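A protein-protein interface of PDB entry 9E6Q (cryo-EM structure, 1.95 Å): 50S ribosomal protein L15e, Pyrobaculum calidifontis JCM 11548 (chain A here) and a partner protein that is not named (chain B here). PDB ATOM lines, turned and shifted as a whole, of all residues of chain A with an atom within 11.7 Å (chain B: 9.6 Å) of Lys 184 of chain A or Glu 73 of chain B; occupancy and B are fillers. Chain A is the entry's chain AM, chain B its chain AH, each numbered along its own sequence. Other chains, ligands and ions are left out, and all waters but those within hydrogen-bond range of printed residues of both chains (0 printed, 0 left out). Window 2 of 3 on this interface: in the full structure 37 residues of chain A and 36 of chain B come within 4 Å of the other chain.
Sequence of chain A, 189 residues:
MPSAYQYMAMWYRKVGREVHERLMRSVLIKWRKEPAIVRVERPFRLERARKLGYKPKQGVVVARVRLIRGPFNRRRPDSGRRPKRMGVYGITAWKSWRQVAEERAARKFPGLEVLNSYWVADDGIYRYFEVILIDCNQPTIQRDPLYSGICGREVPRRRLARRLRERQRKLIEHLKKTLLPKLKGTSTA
The backbone carbonyl oxygen of Leu 72 of chain B sits at hydrogen-bond distance from the side-chain amino group of Lys 176 of chain A, at 3.2 Å. The side-chain carboxylate (OE2) of Glu 73 of chain B is in salt-bridge range of the side-chain amino group (NZ) of Lys 184 of chain A, 3.1 Å away.
OE1 of Glu 73 of chain B is in salt-bridge range of NZ of Lys 75 of chain B. O of Leu 175 of chain A sits at hydrogen-bond distance from N of Leu 180 of chain A, 3.1 Å away.
Ile 172 of chain A touches Leu 72 of chain B (O to CD2, 3.8 Å). Ile 172 of chain A touches Pro 78 of chain B. Leu 72 of chain B touches Leu 175 of chain A (CD2 to CB, 3.7 Å). NZ of Lys 176 of chain A touches O of Val 71 of chain B (3.9 Å). CD2 of Leu 179 of chain A touches O of Val 35 of chain B (3.7 Å). CD2 of Leu 180 of chain A touches O of Leu 72 of chain B, 3.7 Å away. Lys 182 of chain A touches Glu 34 of chain B. Leu 183 of chain A touches Arg 65 of chain B. Leu 183 of chain A touches Leu 68 of chain B (CD1 to CB, 3.7 Å). CD1 of Leu 72 of chain B touches CD1 of Leu 183 of chain A (3.9 Å).
Of chain B, only Glu 73 comes within 4 Å of Lys 184 of chain A. Printed residues of chain A within 4 Å of Glu 73 of chain B: Lys 184. No residue of chain B comes within 4 Å of Gly 185 of chain A. Of chain A, only Lys 176 comes within 4 Å of Val 71 of chain B. Leu 72 of chain B touches just these residues of chain A: Ile 172, Leu 175, Lys 176, Leu 180 and Leu 183. No residue of chain A comes within 4 Å of Gly 74 of chain B. No residue of chain A comes within 4 Å of Lys 75 of chain B. Of the printed residues of chain B, Lys 182 of chain A touches Glu 34 (3.8 Å). Of the printed residues of chain A, Pro 78 of chain B touches Ile 172. Printed residues of chain A within 4 Å of Arg 65 of chain B: Leu 183. Printed residues of chain A within 4 Å of Leu 68 of chain B: Leu 183 (3.7 Å). Of the printed residues of chain B, Leu 179 of chain A touches Val 35. Ile 69 of chain B touches none of the printed residues of chain A. Leu 171 of chain A touches none of the printed residues of chain B. The nearest residue of chain A that does not touch Glu 73 of chain B is Leu 180 of chain A (4.1 Å).
Printed residues of chain B that touch a printed residue of chain A: Glu 34, Val 35, Arg 65, Leu 68, Val 71, Leu 72, Glu 73 and Pro 78. Of the 16 printed residues of chain A, 8 touch a printed residue of chain B. Along chain A the printed residues that touch a printed residue of chain B span positions 172 to 184.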
ATOM      1  N   ARG A 169     -37.565   9.321   4.594  1.00  0.00           N
ATOM      2  CA  ARG A 169     -38.017   8.640   5.801  1.00  0.00           C
ATOM      3  C   ARG A 169     -38.089   7.133   5.591  1.00  0.00           C
ATOM      4  O   ARG A 169     -37.682   6.359   6.460  1.00  0.00           O
ATOM      5  CB  ARG A 169     -39.372   9.196   6.232  1.00  0.00           C
ATOM      6  CG  ARG A 169     -40.134   8.307   7.191  1.00  0.00           C
ATOM      7  CD  ARG A 169     -41.457   8.934   7.596  1.00  0.00           C
ATOM      8  NE  ARG A 169     -42.421   8.945   6.504  1.00  0.00           N
ATOM      9  CZ  ARG A 169     -42.927  10.045   5.964  1.00  0.00           C
ATOM     10  NH1 ARG A 169     -42.563  11.250   6.377  1.00  0.00           N
ATOM     11  NH2 ARG A 169     -43.813   9.936   4.981  1.00  0.00           N
ATOM     12  N   LEU A 171     -36.375   5.380   3.400  1.00  0.00           N
ATOM     13  CA  LEU A 171     -35.036   4.840   3.199  1.00  0.00           C
ATOM     14  C   LEU A 171     -34.340   4.575   4.527  1.00  0.00           C
ATOM     15  O   LEU A 171     -33.669   3.551   4.689  1.00  0.00           O
ATOM     16  CB  LEU A 171     -34.209   5.799   2.345  1.00  0.00           C
ATOM     17  CG  LEU A 171     -32.721   5.481   2.217  1.00  0.00           C
ATOM     18  CD1 LEU A 171     -32.506   4.361   1.225  1.00  0.00           C
ATOM     19  CD2 LEU A 171     -31.929   6.708   1.818  1.00  0.00           C
ATOM     20  N   ILE A 172     -34.484   5.488   5.487  1.00  0.00           N
ATOM     21  CA  ILE A 172     -33.811   5.333   6.771  1.00  0.00           C
ATOM     22  C   ILE A 172     -34.300   4.076   7.479  1.00  0.00           C
ATOM     23  O   ILE A 172     -33.513   3.339   8.083  1.00  0.00           O
ATOM     24  CB  ILE A 172     -34.015   6.593   7.630  1.00  0.00           C
ATOM     25  CG1 ILE A 172     -33.017   7.673   7.224  1.00  0.00           C
ATOM     26  CG2 ILE A 172     -33.873   6.277   9.106  1.00  0.00           C
ATOM     27  CD1 ILE A 172     -33.533   9.070   7.392  1.00  0.00           C
ATOM     28  N   GLU A 173     -35.601   3.806   7.410  1.00  0.00           N
ATOM     29  CA  GLU A 173     -36.134   2.596   8.022  1.00  0.00           C
ATOM     30  C   GLU A 173     -35.576   1.348   7.353  1.00  0.00           C
ATOM     31  O   GLU A 173     -35.235   0.370   8.025  1.00  0.00           O
ATOM     32  CB  GLU A 173     -37.658   2.610   7.960  1.00  0.00           C
ATOM     33  CG  GLU A 173     -38.301   3.726   8.774  1.00  0.00           C
ATOM     34  CD  GLU A 173     -37.556   4.065  10.064  1.00  0.00           C
ATOM     35  OE1 GLU A 173     -37.495   5.262  10.411  1.00  0.00           O
ATOM     36  OE2 GLU A 173     -37.091   3.143  10.769  1.00  0.00           O
ATOM     37  N   HIS A 174     -35.479   1.361   6.026  1.00  0.00           N
ATOM     38  CA  HIS A 174     -34.925   0.216   5.318  1.00  0.00           C
ATOM     39  C   HIS A 174     -33.458   0.009   5.669  1.00  0.00           C
ATOM     40  O   HIS A 174     -33.015  -1.122   5.893  1.00  0.00           O
ATOM     41  CB  HIS A 174     -35.091   0.405   3.816  1.00  0.00           C
ATOM     42  CG  HIS A 174     -34.353  -0.604   3.002  1.00  0.00           C
ATOM     43  ND1 HIS A 174     -33.194  -0.307   2.320  1.00  0.00           N
ATOM     44  CD2 HIS A 174     -34.611  -1.908   2.758  1.00  0.00           C
ATOM     45  CE1 HIS A 174     -32.768  -1.387   1.694  1.00  0.00           C
ATOM     46  NE2 HIS A 174     -33.610  -2.373   1.942  1.00  0.00           N
ATOM     47  N   LEU A 175     -32.681   1.092   5.707  1.00  0.00           N
ATOM     48  CA  LEU A 175     -31.258   0.975   5.989  1.00  0.00           C
ATOM     49  C   LEU A 175     -30.989   0.542   7.421  1.00  0.00           C
ATOM     50  O   LEU A 175     -29.920  -0.008   7.697  1.00  0.00           O
ATOM     51  CB  LEU A 175     -30.553   2.298   5.711  1.00  0.00           C
ATOM     52  CG  LEU A 175     -30.498   2.787   4.265  1.00  0.00           C
ATOM     53  CD1 LEU A 175     -29.762   4.104   4.211  1.00  0.00           C
ATOM     54  CD2 LEU A 175     -29.849   1.766   3.352  1.00  0.00           C
ATOM     55  N   LYS A 176     -31.933   0.778   8.331  1.00  0.00           N
ATOM     56  CA  LYS A 176     -31.775   0.312   9.701  1.00  0.00           C
ATOM     57  C   LYS A 176     -31.667  -1.205   9.745  1.00  0.00           C
ATOM     58  O   LYS A 176     -30.851  -1.764  10.484  1.00  0.00           O
ATOM     59  CB  LYS A 176     -32.951   0.790  10.547  1.00  0.00           C
ATOM     60  CG  LYS A 176     -32.669   2.025  11.362  1.00  0.00           C
ATOM     61  CD  LYS A 176     -33.945   2.785  11.644  1.00  0.00           C
ATOM     62  CE  LYS A 176     -33.825   3.620  12.903  1.00  0.00           C
ATOM     63  NZ  LYS A 176     -33.435   5.028  12.630  1.00  0.00           N
ATOM     64  N   LYS A 177     -32.480  -1.886   8.942  1.00  0.00           N
ATOM     65  CA  LYS A 177     -32.462  -3.342   8.923  1.00  0.00           C
ATOM     66  C   LYS A 177     -31.273  -3.873   8.131  1.00  0.00           C
ATOM     67  O   LYS A 177     -30.512  -4.713   8.621  1.00  0.00           O
ATOM     68  CB  LYS A 177     -33.769  -3.857   8.332  1.00  0.00           C
ATOM     69  CG  LYS A 177     -34.952  -3.789   9.281  1.00  0.00           C
ATOM     70  CD  LYS A 177     -36.216  -3.320   8.575  1.00  0.00           C
ATOM     71  CE  LYS A 177     -36.418  -3.992   7.226  1.00  0.00           C
ATOM     72  NZ  LYS A 177     -36.242  -5.468   7.256  1.00  0.00           N
ATOM     73  N   THR A 178     -31.095  -3.393   6.908  1.00  0.00           N
ATOM     74  CA  THR A 178     -30.166  -4.008   5.976  1.00  0.00           C
ATOM     75  C   THR A 178     -28.772  -3.401   5.993  1.00  0.00           C
ATOM     76  O   THR A 178     -27.878  -3.935   5.331  1.00  0.00           O
ATOM     77  CB  THR A 178     -30.725  -3.920   4.556  1.00  0.00           C
ATOM     78  OG1 THR A 178     -31.055  -2.561   4.261  1.00  0.00           O
ATOM     79  CG2 THR A 178     -31.975  -4.768   4.433  1.00  0.00           C
ATOM     80  N   LEU A 179     -28.555  -2.321   6.707  1.00  0.00           N
ATOM     81  CA  LEU A 179     -27.228  -1.723   6.626  1.00  0.00           C
ATOM     82  C   LEU A 179     -26.589  -1.482   7.980  1.00  0.00           C
ATOM     83  O   LEU A 179     -25.377  -1.646   8.111  1.00  0.00           O
ATOM     84  CB  LEU A 179     -27.286  -0.403   5.852  1.00  0.00           C
ATOM     85  CG  LEU A 179     -25.929   0.233   5.551  1.00  0.00           C
ATOM     86  CD1 LEU A 179     -25.132  -0.657   4.629  1.00  0.00           C
ATOM     87  CD2 LEU A 179     -26.095   1.621   4.962  1.00  0.00           C
ATOM     88  N   LEU A 180     -27.368  -1.094   8.985  1.00  0.00           N
ATOM     89  CA  LEU A 180     -26.797  -0.792  10.294  1.00  0.00           C
ATOM     90  C   LEU A 180     -25.965  -1.928  10.875  1.00  0.00           C
ATOM     91  O   LEU A 180     -24.886  -1.640  11.419  1.00  0.00           O
ATOM     92  CB  LEU A 180     -27.915  -0.381  11.262  1.00  0.00           C
ATOM     93  CG  LEU A 180     -27.483   0.059  12.657  1.00  0.00           C
ATOM     94  CD1 LEU A 180     -26.444   1.154  12.570  1.00  0.00           C
ATOM     95  CD2 LEU A 180     -28.685   0.542  13.435  1.00  0.00           C
ATOM     96  N   PRO A 181     -26.379  -3.199  10.822  1.00  0.00           N
ATOM     97  CA  PRO A 181     -25.473  -4.260  11.296  1.00  0.00           C
ATOM     98  C   PRO A 181     -24.155  -4.317  10.543  1.00  0.00           C
ATOM     99  O   PRO A 181     -23.101  -4.502  11.161  1.00  0.00           O
ATOM    100  CB  PRO A 181     -26.301  -5.534  11.099  1.00  0.00           C
ATOM    101  CG  PRO A 181     -27.704  -5.084  11.089  1.00  0.00           C
ATOM    102  CD  PRO A 181     -27.704  -3.732  10.465  1.00  0.00           C
ATOM    103  N   LYS A 182     -24.182  -4.148   9.220  1.00  0.00           N
ATOM    104  CA  LYS A 182     -22.948  -4.235   8.448  1.00  0.00           C
ATOM    105  C   LYS A 182     -22.006  -3.089   8.790  1.00  0.00           C
ATOM    106  O   LYS A 182     -20.787  -3.276   8.848  1.00  0.00           O
ATOM    107  CB  LYS A 182     -23.257  -4.247   6.953  1.00  0.00           C
ATOM    108  CG  LYS A 182     -22.264  -5.048   6.128  1.00  0.00           C
ATOM    109  CD  LYS A 182     -21.205  -4.154   5.496  1.00  0.00           C
ATOM    110  CE  LYS A 182     -21.642  -3.641   4.133  1.00  0.00           C
ATOM    111  NZ  LYS A 182     -20.577  -2.823   3.489  1.00  0.00           N
ATOM    112  N   LEU A 183     -22.552  -1.892   9.011  1.00  0.00           N
ATOM    113  CA  LEU A 183     -21.719  -0.755   9.383  1.00  0.00           C
ATOM    114  C   LEU A 183     -21.040  -0.987  10.725  1.00  0.00           C
ATOM    115  O   LEU A 183     -19.851  -0.696  10.890  1.00  0.00           O
ATOM    116  CB  LEU A 183     -22.558   0.519   9.425  1.00  0.00           C
ATOM    117  CG  LEU A 183     -22.984   1.081   8.070  1.00  0.00           C
ATOM    118  CD1 LEU A 183     -23.907   2.264   8.263  1.00  0.00           C
ATOM    119  CD2 LEU A 183     -21.768   1.470   7.249  1.00  0.00           C
ATOM    120  N   LYS A 184     -21.785  -1.510  11.697  1.00  0.00           N
ATOM    121  CA  LYS A 184     -21.248  -1.742  13.030  1.00  0.00           C
ATOM    122  C   LYS A 184     -20.488  -3.054  13.149  1.00  0.00           C
ATOM    123  O   LYS A 184     -19.808  -3.262  14.157  1.00  0.00           O
ATOM    124  CB  LYS A 184     -22.375  -1.718  14.063  1.00  0.00           C
ATOM    125  CG  LYS A 184     -22.230  -0.618  15.097  1.00  0.00           C
ATOM    126  CD  LYS A 184     -23.183  -0.824  16.252  1.00  0.00           C
ATOM    127  CE  LYS A 184     -24.561  -0.310  15.905  1.00  0.00           C
ATOM    128  NZ  LYS A 184     -25.597  -0.802  16.849  1.00  0.00           N
ATOM    129  N   GLY A 185     -20.591  -3.935  12.163  1.00  0.00           N
ATOM    130  CA  GLY A 185     -19.901  -5.210  12.207  1.00  0.00           C
ATOM    131  C   GLY A 185     -18.432  -5.097  11.854  1.00  0.00           C
ATOM    132  O   GLY A 185     -17.807  -6.071  11.434  1.00  0.00           O
ATOM    133  N   GLU B  34     -18.178   1.752  -0.260  1.00  0.00           N
ATOM    134  CA  GLU B  34     -17.603   1.074   0.895  1.00  0.00           C
ATOM    135  C   GLU B  34     -18.530   1.118   2.100  1.00  0.00           C
ATOM    136  O   GLU B  34     -18.424   0.270   2.990  1.00  0.00           O
ATOM    137  CB  GLU B  34     -16.247   1.686   1.233  1.00  0.00           C
ATOM    138  CG  GLU B  34     -15.171   1.300   0.242  1.00  0.00           C
ATOM    139  CD  GLU B  34     -13.783   1.685   0.696  1.00  0.00           C
ATOM    140  OE1 GLU B  34     -13.567   1.836   1.914  1.00  0.00           O
ATOM    141  OE2 GLU B  34     -12.900   1.836  -0.170  1.00  0.00           O
ATOM    142  N   VAL B  35     -19.444   2.084   2.151  1.00  0.00           N
ATOM    143  CA  VAL B  35     -20.443   2.140   3.208  1.00  0.00           C
ATOM    144  C   VAL B  35     -21.802   1.642   2.726  1.00  0.00           C
ATOM    145  O   VAL B  35     -22.815   1.900   3.375  1.00  0.00           O
ATOM    146  CB  VAL B  35     -20.550   3.556   3.795  1.00  0.00           C
ATOM    147  CG1 VAL B  35     -19.331   3.876   4.633  1.00  0.00           C
ATOM    148  CG2 VAL B  35     -20.717   4.579   2.697  1.00  0.00           C
ATOM    149  N   ARG B  65     -18.894   6.417   7.703  1.00  0.00           N
ATOM    150  CA  ARG B  65     -19.353   5.315   8.541  1.00  0.00           C
ATOM    151  C   ARG B  65     -19.783   5.808   9.913  1.00  0.00           C
ATOM    152  O   ARG B  65     -20.796   5.353  10.453  1.00  0.00           O
ATOM    153  CB  ARG B  65     -18.262   4.258   8.676  1.00  0.00           C
ATOM    154  CG  ARG B  65     -18.761   2.960   9.273  1.00  0.00           C
ATOM    155  CD  ARG B  65     -17.622   2.035   9.621  1.00  0.00           C
ATOM    156  NE  ARG B  65     -16.495   2.196   8.714  1.00  0.00           N
ATOM    157  CZ  ARG B  65     -16.358   1.552   7.563  1.00  0.00           C
ATOM    158  NH1 ARG B  65     -17.276   0.706   7.131  1.00  0.00           N
ATOM    159  NH2 ARG B  65     -15.272   1.764   6.828  1.00  0.00           N
ATOM    160  N   LYS B  66     -19.028   6.738  10.491  1.00  0.00           N
ATOM    161  CA  LYS B  66     -19.359   7.248  11.814  1.00  0.00           C
ATOM    162  C   LYS B  66     -20.701   7.965  11.808  1.00  0.00           C
ATOM    163  O   LYS B  66     -21.534   7.756  12.694  1.00  0.00           O
ATOM    164  CB  LYS B  66     -18.251   8.178  12.298  1.00  0.00           C
ATOM    165  CG  LYS B  66     -18.282   8.456  13.781  1.00  0.00           C
ATOM    166  CD  LYS B  66     -18.787   9.856  14.069  1.00  0.00           C
ATOM    167  CE  LYS B  66     -18.207  10.400  15.363  1.00  0.00           C
ATOM    168  NZ  LYS B  66     -18.345  11.879  15.443  1.00  0.00           N
ATOM    169  N   TRP B  67     -20.932   8.809  10.803  1.00  0.00           N
ATOM    170  CA  TRP B  67     -22.145   9.618  10.777  1.00  0.00           C
ATOM    171  C   TRP B  67     -23.364   8.788  10.406  1.00  0.00           C
ATOM    172  O   TRP B  67     -24.470   9.057  10.884  1.00  0.00           O
ATOM    173  CB  TRP B  67     -21.981  10.779   9.804  1.00  0.00           C
ATOM    174  CG  TRP B  67     -23.213  11.596   9.663  1.00  0.00           C
ATOM    175  CD1 TRP B  67     -23.647  12.568  10.503  1.00  0.00           C
ATOM    176  CD2 TRP B  67     -24.183  11.507   8.617  1.00  0.00           C
ATOM    177  NE1 TRP B  67     -24.825  13.094  10.050  1.00  0.00           N
ATOM    178  CE2 TRP B  67     -25.177  12.458   8.891  1.00  0.00           C
ATOM    179  CE3 TRP B  67     -24.305  10.714   7.476  1.00  0.00           C
ATOM    180  CZ2 TRP B  67     -26.277  12.645   8.062  1.00  0.00           C
ATOM    181  CZ3 TRP B  67     -25.397  10.899   6.657  1.00  0.00           C
ATOM    182  CH2 TRP B  67     -26.370  11.854   6.955  1.00  0.00           C
ATOM    183  N   LEU B  68     -23.190   7.794   9.536  1.00  0.00           N
ATOM    184  CA  LEU B  68     -24.310   6.938   9.167  1.00  0.00           C
ATOM    185  C   LEU B  68     -24.826   6.166  10.369  1.00  0.00           C
ATOM    186  O   LEU B  68     -26.038   5.997  10.532  1.00  0.00           O
ATOM    187  CB  LEU B  68     -23.899   5.980   8.053  1.00  0.00           C
ATOM    188  CG  LEU B  68     -23.838   6.579   6.650  1.00  0.00           C
ATOM    189  CD1 LEU B  68     -23.300   5.561   5.673  1.00  0.00           C
ATOM    190  CD2 LEU B  68     -25.208   7.060   6.219  1.00  0.00           C
ATOM    191  N   ILE B  69     -23.918   5.692  11.221  1.00  0.00           N
ATOM    192  CA  ILE B  69     -24.329   4.969  12.420  1.00  0.00           C
ATOM    193  C   ILE B  69     -25.164   5.870  13.319  1.00  0.00           C
ATOM    194  O   ILE B  69     -26.207   5.462  13.838  1.00  0.00           O
ATOM    195  CB  ILE B  69     -23.095   4.414  13.153  1.00  0.00           C
ATOM    196  CG1 ILE B  69     -22.599   3.150  12.453  1.00  0.00           C
ATOM    197  CG2 ILE B  69     -23.406   4.144  14.612  1.00  0.00           C
ATOM    198  CD1 ILE B  69     -21.224   2.726  12.864  1.00  0.00           C
ATOM    199  N   GLU B  70     -24.738   7.121  13.487  1.00  0.00           N
ATOM    200  CA  GLU B  70     -25.520   8.063  14.277  1.00  0.00           C
ATOM    201  C   GLU B  70     -26.906   8.266  13.683  1.00  0.00           C
ATOM    202  O   GLU B  70     -27.898   8.342  14.414  1.00  0.00           O
ATOM    203  CB  GLU B  70     -24.786   9.397  14.385  1.00  0.00           C
ATOM    204  CG  GLU B  70     -23.644   9.396  15.374  1.00  0.00           C
ATOM    205  CD  GLU B  70     -22.681  10.549  15.156  1.00  0.00           C
ATOM    206  OE1 GLU B  70     -23.067  11.535  14.496  1.00  0.00           O
ATOM    207  OE2 GLU B  70     -21.538  10.472  15.650  1.00  0.00           O
ATOM    208  N   VAL B  71     -26.997   8.362  12.358  1.00  0.00           N
ATOM    209  CA  VAL B  71     -28.285   8.584  11.711  1.00  0.00           C
ATOM    210  C   VAL B  71     -29.179   7.361  11.855  1.00  0.00           C
ATOM    211  O   VAL B  71     -30.369   7.474  12.166  1.00  0.00           O
ATOM    212  CB  VAL B  71     -28.079   8.959  10.234  1.00  0.00           C
ATOM    213  CG1 VAL B  71     -29.353   8.742   9.443  1.00  0.00           C
ATOM    214  CG2 VAL B  71     -27.641  10.388  10.131  1.00  0.00           C
ATOM    215  N   LEU B  72     -28.622   6.175  11.626  1.00  0.00           N
ATOM    216  CA  LEU B  72     -29.435   4.970  11.643  1.00  0.00           C
ATOM    217  C   LEU B  72     -29.796   4.535  13.056  1.00  0.00           C
ATOM    218  O   LEU B  72     -30.624   3.635  13.221  1.00  0.00           O
ATOM    219  CB  LEU B  72     -28.712   3.854  10.894  1.00  0.00           C
ATOM    220  CG  LEU B  72     -28.553   4.145   9.399  1.00  0.00           C
ATOM    221  CD1 LEU B  72     -27.747   3.076   8.692  1.00  0.00           C
ATOM    222  CD2 LEU B  72     -29.906   4.307   8.747  1.00  0.00           C
ATOM    223  N   GLU B  73     -29.198   5.143  14.075  1.00  0.00           N
ATOM    224  CA  GLU B  73     -29.568   4.897  15.461  1.00  0.00           C
ATOM    225  C   GLU B  73     -30.425   6.006  16.048  1.00  0.00           C
ATOM    226  O   GLU B  73     -30.683   5.999  17.254  1.00  0.00           O
ATOM    227  CB  GLU B  73     -28.316   4.715  16.316  1.00  0.00           C
ATOM    228  CG  GLU B  73     -27.453   3.560  15.883  1.00  0.00           C
ATOM    229  CD  GLU B  73     -26.232   3.408  16.749  1.00  0.00           C
ATOM    230  OE1 GLU B  73     -25.718   4.433  17.240  1.00  0.00           O
ATOM    231  OE2 GLU B  73     -25.776   2.268  16.935  1.00  0.00           O
ATOM    232  N   GLY B  74     -30.857   6.963  15.236  1.00  0.00           N
ATOM    233  CA  GLY B  74     -31.708   8.027  15.717  1.00  0.00           C
ATOM    234  C   GLY B  74     -31.008   9.122  16.484  1.00  0.00           C
ATOM    235  O   GLY B  74     -31.686   9.941  17.109  1.00  0.00           O
ATOM    236  N   LYS B  75     -29.676   9.165  16.464  1.00  0.00           N
ATOM    237  CA  LYS B  75     -28.937  10.194  17.183  1.00  0.00           C
ATOM    238  C   LYS B  75     -28.657  11.432  16.346  1.00  0.00           C
ATOM    239  O   LYS B  75     -28.413  12.501  16.915  1.00  0.00           O
ATOM    240  CB  LYS B  75     -27.607   9.635  17.692  1.00  0.00           C
ATOM    241  CG  LYS B  75     -27.728   8.340  18.462  1.00  0.00           C
ATOM    242  CD  LYS B  75     -27.020   8.440  19.792  1.00  0.00           C
ATOM    243  CE  LYS B  75     -26.796   7.068  20.398  1.00  0.00           C
ATOM    244  NZ  LYS B  75     -26.316   6.081  19.394  1.00  0.00           N
ATOM    245  N   ALA B  76     -28.677  11.318  15.025  1.00  0.00           N
ATOM    246  CA  ALA B  76     -28.449  12.450  14.145  1.00  0.00           C
ATOM    247  C   ALA B  76     -29.607  12.565  13.170  1.00  0.00           C
ATOM    248  O   ALA B  76     -30.161  11.557  12.729  1.00  0.00           O
ATOM    249  CB  ALA B  76     -27.128  12.312  13.382  1.00  0.00           C
ATOM    250  N   THR B  77     -29.975  13.800  12.846  1.00  0.00           N
ATOM    251  CA  THR B  77     -31.037  14.049  11.889  1.00  0.00           C
ATOM    252  C   THR B  77     -30.426  14.403  10.547  1.00  0.00           C
ATOM    253  O   THR B  77     -29.701  15.405  10.457  1.00  0.00           O
ATOM    254  CB  THR B  77     -31.941  15.175  12.365  1.00  0.00           C
ATOM    255  OG1 THR B  77     -32.050  15.127  13.790  1.00  0.00           O
ATOM    256  CG2 THR B  77     -33.318  15.026  11.761  1.00  0.00           C
ATOM    257  N   PRO B  78     -30.666  13.626   9.501  1.00  0.00           N
ATOM    258  CA  PRO B  78     -30.152  13.984   8.189  1.00  0.00           C
ATOM    259  C   PRO B  78     -30.763  15.289   7.719  1.00  0.00           C
ATOM    260  O   PRO B  78     -31.937  15.569   7.994  1.00  0.00           O
ATOM    261  CB  PRO B  78     -30.592  12.812   7.301  1.00  0.00           C
ATOM    262  CG  PRO B  78     -31.727  12.205   7.997  1.00  0.00           C
ATOM    263  CD  PRO B  78     -31.573  12.469   9.455  1.00  0.00           C
